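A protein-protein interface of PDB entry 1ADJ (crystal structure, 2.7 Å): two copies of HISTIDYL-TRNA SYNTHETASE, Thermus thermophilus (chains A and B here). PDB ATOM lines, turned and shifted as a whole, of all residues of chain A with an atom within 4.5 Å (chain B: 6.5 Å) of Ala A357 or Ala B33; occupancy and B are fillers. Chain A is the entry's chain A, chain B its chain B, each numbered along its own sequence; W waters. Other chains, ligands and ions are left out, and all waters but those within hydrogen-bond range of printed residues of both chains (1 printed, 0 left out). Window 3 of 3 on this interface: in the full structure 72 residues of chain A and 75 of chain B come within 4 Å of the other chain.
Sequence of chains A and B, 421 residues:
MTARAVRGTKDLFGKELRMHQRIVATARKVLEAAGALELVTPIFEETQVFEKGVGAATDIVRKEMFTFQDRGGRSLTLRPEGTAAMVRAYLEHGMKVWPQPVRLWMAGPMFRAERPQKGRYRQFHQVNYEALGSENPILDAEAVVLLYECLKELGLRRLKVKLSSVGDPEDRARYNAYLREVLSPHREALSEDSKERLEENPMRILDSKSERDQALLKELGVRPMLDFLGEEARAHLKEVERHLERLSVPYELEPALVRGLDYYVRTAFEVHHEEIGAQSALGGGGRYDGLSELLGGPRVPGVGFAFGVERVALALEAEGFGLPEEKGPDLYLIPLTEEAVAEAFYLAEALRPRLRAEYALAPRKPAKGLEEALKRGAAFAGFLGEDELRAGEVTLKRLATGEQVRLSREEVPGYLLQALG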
ATOM      1  N   LEU A 331       4.225   3.375   0.510  1.00  0.00           N
ATOM      2  CA  LEU A 331       5.545   2.772   0.427  1.00  0.00           C
ATOM      3  C   LEU A 331       5.926   2.441  -1.007  1.00  0.00           C
ATOM      4  O   LEU A 331       5.088   1.996  -1.795  1.00  0.00           O
ATOM      5  CB  LEU A 331       5.581   1.483   1.245  1.00  0.00           C
ATOM      6  CG  LEU A 331       6.860   0.660   1.153  1.00  0.00           C
ATOM      7  CD1 LEU A 331       7.982   1.386   1.869  1.00  0.00           C
ATOM      8  CD2 LEU A 331       6.618  -0.695   1.771  1.00  0.00           C
ATOM      9  N   ALA A 348       4.932  -6.215  -1.249  1.00  0.00           N
ATOM     10  CA  ALA A 348       3.907  -5.246  -1.608  1.00  0.00           C
ATOM     11  C   ALA A 348       2.535  -5.905  -1.483  1.00  0.00           C
ATOM     12  O   ALA A 348       1.632  -5.352  -0.855  1.00  0.00           O
ATOM     13  CB  ALA A 348       4.127  -4.741  -3.028  1.00  0.00           C
ATOM     14  N   LEU A 351       1.181  -6.214   1.997  1.00  0.00           N
ATOM     15  CA  LEU A 351       0.766  -4.932   2.551  1.00  0.00           C
ATOM     16  C   LEU A 351      -0.563  -4.401   2.005  1.00  0.00           C
ATOM     17  O   LEU A 351      -1.272  -3.671   2.703  1.00  0.00           O
ATOM     18  CB  LEU A 351       1.859  -3.896   2.315  1.00  0.00           C
ATOM     19  CG  LEU A 351       3.234  -4.285   2.838  1.00  0.00           C
ATOM     20  CD1 LEU A 351       4.258  -3.244   2.435  1.00  0.00           C
ATOM     21  CD2 LEU A 351       3.181  -4.437   4.340  1.00  0.00           C
ATOM     22  N   ARG A 352      -0.889  -4.742   0.759  1.00  0.00           N
ATOM     23  CA  ARG A 352      -2.136  -4.290   0.126  1.00  0.00           C
ATOM     24  C   ARG A 352      -3.331  -5.143   0.536  1.00  0.00           C
ATOM     25  O   ARG A 352      -3.175  -6.320   0.861  1.00  0.00           O
ATOM     26  CB  ARG A 352      -2.030  -4.375  -1.386  1.00  0.00           C
ATOM     27  CG  ARG A 352      -0.874  -3.657  -2.007  1.00  0.00           C
ATOM     28  CD  ARG A 352      -0.633  -4.351  -3.316  1.00  0.00           C
ATOM     29  NE  ARG A 352       0.347  -3.692  -4.164  1.00  0.00           N
ATOM     30  CZ  ARG A 352       0.754  -4.195  -5.324  1.00  0.00           C
ATOM     31  NH1 ARG A 352       0.262  -5.356  -5.739  1.00  0.00           N
ATOM     32  NH2 ARG A 352       1.605  -3.523  -6.085  1.00  0.00           N
ATOM     33  N   PRO A 353      -4.553  -4.581   0.463  1.00  0.00           N
ATOM     34  CA  PRO A 353      -4.850  -3.215   0.023  1.00  0.00           C
ATOM     35  C   PRO A 353      -4.928  -2.189   1.167  1.00  0.00           C
ATOM     36  O   PRO A 353      -5.154  -1.009   0.919  1.00  0.00           O
ATOM     37  CB  PRO A 353      -6.198  -3.385  -0.658  1.00  0.00           C
ATOM     38  CG  PRO A 353      -6.872  -4.357   0.241  1.00  0.00           C
ATOM     39  CD  PRO A 353      -5.793  -5.380   0.539  1.00  0.00           C
ATOM     40  N   LEU A 355      -2.674  -0.931   2.757  1.00  0.00           N
ATOM     41  CA  LEU A 355      -1.586   0.012   2.544  1.00  0.00           C
ATOM     42  C   LEU A 355      -1.342   0.076   1.045  1.00  0.00           C
ATOM     43  O   LEU A 355      -1.510  -0.923   0.346  1.00  0.00           O
ATOM     44  CB  LEU A 355      -0.327  -0.508   3.240  1.00  0.00           C
ATOM     45  CG  LEU A 355       0.370   0.331   4.303  1.00  0.00           C
ATOM     46  CD1 LEU A 355      -0.627   1.119   5.107  1.00  0.00           C
ATOM     47  CD2 LEU A 355       1.167  -0.596   5.195  1.00  0.00           C
ATOM     48  N   ARG A 356      -1.013   1.259   0.540  1.00  0.00           N
ATOM     49  CA  ARG A 356      -0.740   1.408  -0.880  1.00  0.00           C
ATOM     50  C   ARG A 356       0.753   1.225  -1.050  1.00  0.00           C
ATOM     51  O   ARG A 356       1.539   2.120  -0.706  1.00  0.00           O
ATOM     52  CB  ARG A 356      -1.163   2.776  -1.392  1.00  0.00           C
ATOM     53  CG  ARG A 356      -0.776   2.990  -2.840  1.00  0.00           C
ATOM     54  CD  ARG A 356      -1.345   4.269  -3.392  1.00  0.00           C
ATOM     55  NE  ARG A 356      -0.771   4.583  -4.695  1.00  0.00           N
ATOM     56  CZ  ARG A 356      -0.898   5.758  -5.305  1.00  0.00           C
ATOM     57  NH1 ARG A 356      -1.596   6.732  -4.732  1.00  0.00           N
ATOM     58  NH2 ARG A 356      -0.276   5.983  -6.459  1.00  0.00           N
ATOM     59  N   ALA A 357       1.131   0.063  -1.585  1.00  0.00           N
ATOM     60  CA  ALA A 357       2.527  -0.297  -1.783  1.00  0.00           C
ATOM     61  C   ALA A 357       2.860  -0.536  -3.244  1.00  0.00           C
ATOM     62  O   ALA A 357       2.177  -1.297  -3.934  1.00  0.00           O
ATOM     63  CB  ALA A 357       2.860  -1.538  -0.961  1.00  0.00           C
ATOM     64  N   GLU A 358       3.917   0.116  -3.703  1.00  0.00           N
ATOM     65  CA  GLU A 358       4.384  -0.014  -5.074  1.00  0.00           C
ATOM     66  C   GLU A 358       5.859  -0.415  -5.042  1.00  0.00           C
ATOM     67  O   GLU A 358       6.500  -0.335  -3.997  1.00  0.00           O
ATOM     68  CB  GLU A 358       4.200   1.303  -5.823  1.00  0.00           C
ATOM     69  CG  GLU A 358       2.758   1.601  -6.191  1.00  0.00           C
ATOM     70  CD  GLU A 358       2.564   3.019  -6.696  1.00  0.00           C
ATOM     71  OE1 GLU A 358       3.351   3.475  -7.554  1.00  0.00           O
ATOM     72  OE2 GLU A 358       1.621   3.684  -6.228  1.00  0.00           O
ATOM     73  N   ARG B  28     -11.837  -0.460  -7.180  1.00  0.00           N
ATOM     74  CA  ARG B  28     -11.073   0.788  -7.149  1.00  0.00           C
ATOM     75  C   ARG B  28     -10.003   0.740  -6.057  1.00  0.00           C
ATOM     76  O   ARG B  28      -8.846   1.106  -6.284  1.00  0.00           O
ATOM     77  CB  ARG B  28     -12.004   1.995  -6.908  1.00  0.00           C
ATOM     78  CG  ARG B  28     -11.273   3.313  -6.579  1.00  0.00           C
ATOM     79  CD  ARG B  28     -12.215   4.513  -6.413  1.00  0.00           C
ATOM     80  NE  ARG B  28     -12.579   5.119  -7.696  1.00  0.00           N
ATOM     81  CZ  ARG B  28     -13.814   5.149  -8.206  1.00  0.00           C
ATOM     82  NH1 ARG B  28     -14.834   4.605  -7.540  1.00  0.00           N
ATOM     83  NH2 ARG B  28     -14.027   5.705  -9.399  1.00  0.00           N
ATOM     84  N   LYS B  29     -10.387   0.262  -4.882  1.00  0.00           N
ATOM     85  CA  LYS B  29      -9.458   0.185  -3.767  1.00  0.00           C
ATOM     86  C   LYS B  29      -8.272  -0.759  -4.024  1.00  0.00           C
ATOM     87  O   LYS B  29      -7.109  -0.349  -3.898  1.00  0.00           O
ATOM     88  CB  LYS B  29     -10.190  -0.217  -2.481  1.00  0.00           C
ATOM     89  CG  LYS B  29      -9.288  -0.216  -1.261  1.00  0.00           C
ATOM     90  CD  LYS B  29     -10.008  -0.643  -0.001  1.00  0.00           C
ATOM     91  CE  LYS B  29      -9.065  -0.562   1.202  1.00  0.00           C
ATOM     92  NZ  LYS B  29      -8.440   0.797   1.343  1.00  0.00           N
ATOM     93  N   VAL B  30      -8.558  -2.000  -4.420  1.00  0.00           N
ATOM     94  CA  VAL B  30      -7.489  -2.963  -4.659  1.00  0.00           C
ATOM     95  C   VAL B  30      -6.591  -2.554  -5.817  1.00  0.00           C
ATOM     96  O   VAL B  30      -5.366  -2.578  -5.690  1.00  0.00           O
ATOM     97  CB  VAL B  30      -8.014  -4.418  -4.881  1.00  0.00           C
ATOM     98  CG1 VAL B  30      -9.031  -4.790  -3.815  1.00  0.00           C
ATOM     99  CG2 VAL B  30      -8.608  -4.581  -6.246  1.00  0.00           C
ATOM    100  N   LEU B  31      -7.199  -2.111  -6.914  1.00  0.00           N
ATOM    101  CA  LEU B  31      -6.462  -1.703  -8.103  1.00  0.00           C
ATOM    102  C   LEU B  31      -5.588  -0.489  -7.871  1.00  0.00           C
ATOM    103  O   LEU B  31      -4.416  -0.483  -8.261  1.00  0.00           O
ATOM    104  CB  LEU B  31      -7.425  -1.452  -9.259  1.00  0.00           C
ATOM    105  CG  LEU B  31      -7.718  -2.614 -10.213  1.00  0.00           C
ATOM    106  CD1 LEU B  31      -7.727  -3.953  -9.507  1.00  0.00           C
ATOM    107  CD2 LEU B  31      -9.050  -2.358 -10.908  1.00  0.00           C
ATOM    108  N   GLU B  32      -6.135   0.526  -7.207  1.00  0.00           N
ATOM    109  CA  GLU B  32      -5.372   1.740  -6.942  1.00  0.00           C
ATOM    110  C   GLU B  32      -4.264   1.548  -5.907  1.00  0.00           C
ATOM    111  O   GLU B  32      -3.263   2.272  -5.917  1.00  0.00           O
ATOM    112  CB  GLU B  32      -6.302   2.892  -6.577  1.00  0.00           C
ATOM    113  CG  GLU B  32      -7.216   3.266  -7.734  1.00  0.00           C
ATOM    114  CD  GLU B  32      -7.860   4.624  -7.586  1.00  0.00           C
ATOM    115  OE1 GLU B  32      -8.047   5.074  -6.438  1.00  0.00           O
ATOM    116  OE2 GLU B  32      -8.186   5.237  -8.625  1.00  0.00           O
ATOM    117  N   ALA B  33      -4.417   0.542  -5.052  1.00  0.00           N
ATOM    118  CA  ALA B  33      -3.400   0.242  -4.051  1.00  0.00           C
ATOM    119  C   ALA B  33      -2.182  -0.333  -4.766  1.00  0.00           C
ATOM    120  O   ALA B  33      -1.058  -0.205  -4.282  1.00  0.00           O
ATOM    121  CB  ALA B  33      -3.930  -0.755  -3.030  1.00  0.00           C
ATOM    122  N   ALA B  34      -2.422  -0.963  -5.920  1.00  0.00           N
ATOM    123  CA  ALA B  34      -1.359  -1.556  -6.725  1.00  0.00           C
ATOM    124  C   ALA B  34      -0.729  -0.526  -7.653  1.00  0.00           C
ATOM    125  O   ALA B  34       0.145  -0.857  -8.454  1.00  0.00           O
ATOM    126  CB  ALA B  34      -1.892  -2.734  -7.523  1.00  0.00           C
ATOM    127  N   GLY B  35      -1.196   0.714  -7.564  1.00  0.00           N
ATOM    128  CA  GLY B  35      -0.648   1.776  -8.383  1.00  0.00           C
ATOM    129  C   GLY B  35      -1.402   2.082  -9.655  1.00  0.00           C
ATOM    130  O   GLY B  35      -0.911   2.840 -10.483  1.00  0.00           O
ATOM    131  N   ALA B  36      -2.589   1.511  -9.825  1.00  0.00           N
ATOM    132  CA  ALA B  36      -3.374   1.760 -11.031  1.00  0.00           C
ATOM    133  C   ALA B  36      -3.984   3.166 -11.055  1.00  0.00           C
ATOM    134  O   ALA B  36      -4.486   3.657 -10.046  1.00  0.00           O
ATOM    135  CB  ALA B  36      -4.465   0.710 -11.176  1.00  0.00           C
ATOM    136  N   GLU B 142       0.670 -10.648 -10.899  1.00  0.00           N
ATOM    137  CA  GLU B 142      -0.002  -9.521 -10.248  1.00  0.00           C
ATOM    138  C   GLU B 142      -1.407  -9.337 -10.781  1.00  0.00           C
ATOM    139  O   GLU B 142      -2.351  -9.183 -10.015  1.00  0.00           O
ATOM    140  CB  GLU B 142       0.794  -8.234 -10.474  1.00  0.00           C
ATOM    141  CG  GLU B 142       0.279  -7.020  -9.704  1.00  0.00           C
ATOM    142  CD  GLU B 142       1.186  -5.805  -9.864  1.00  0.00           C
ATOM    143  OE1 GLU B 142       1.434  -5.395 -11.018  1.00  0.00           O
ATOM    144  OE2 GLU B 142       1.658  -5.261  -8.840  1.00  0.00           O
HETATM  145  O   HOH W   1       2.732  -2.272  -8.188  1.00  0.00           O
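The guanidinium group (NH2) of Arg A352 lies within salt-bridge range of the side-chain carboxylate (OE2) of Glu B142, at 3.3 Å.
N of Ala A357 sits at hydrogen-bond distance from O of Ala B33, 3.5 Å away.
Hydrophobic or aromatic side chains of chain B that line the printed part of chain A: Ala B34.
Among the printed residues, Asp or Glu carboxylates within 4 Å of a Lys or Arg side-chain nitrogen of the other chain: Arg A352 with Glu B142 (3.3 Å).
Water W1 lies within hydrogen-bond range of NH2 of Arg A352 (2.7 Å), O of Ala B34 (3.0 Å) and OE2 of Glu B142 (3.2 Å).
No position is printed for both chains.
Of the 8 pairs that touch across the chains among the printed residues, none has its exchanged pair printed and touching as well.
NE of Arg A352 is in hydrogen-bond range of O of Ala A357, 3.0 Å away.
The backbone NH (N) of Leu A331 is in hydrogen-bond range of the backbone carbonyl oxygen (O) of Arg A356 (3.2 Å).
NE of Arg A356 lies within salt-bridge range of OE2 of Glu A358 (3.0 Å).
The backbone carbonyl oxygen (O) of Leu A331 is in hydrogen-bond range of the backbone NH (N) of Glu A358, at 2.9 Å.
Among the printed residues, pairs that only touch across the chains: Arg A352 with Ala B33, Arg A352 with Ala B34, Pro A353 with Lys B29, Arg A356 with Glu B32, Arg A356 with Ala B33 and Glu A358 with Gly B35.
Ala A357 touches just one residue of chain B: Ala B33 (3.4 Å).
Ala B33 touches just these residues of chain A: Arg A352, Arg A356 and Ala A357.
Printed residues of chain A within 4 Å of Ala B34: Arg A352.
Of the printed residues of chain A, Lys B29 touches Pro A353 (3.8 Å).
Printed residues of chain B within 4 Å of Arg A352: Ala B33, Ala B34 and Glu B142.
Of the printed residues of chain A, Glu B32 touches Arg A356.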
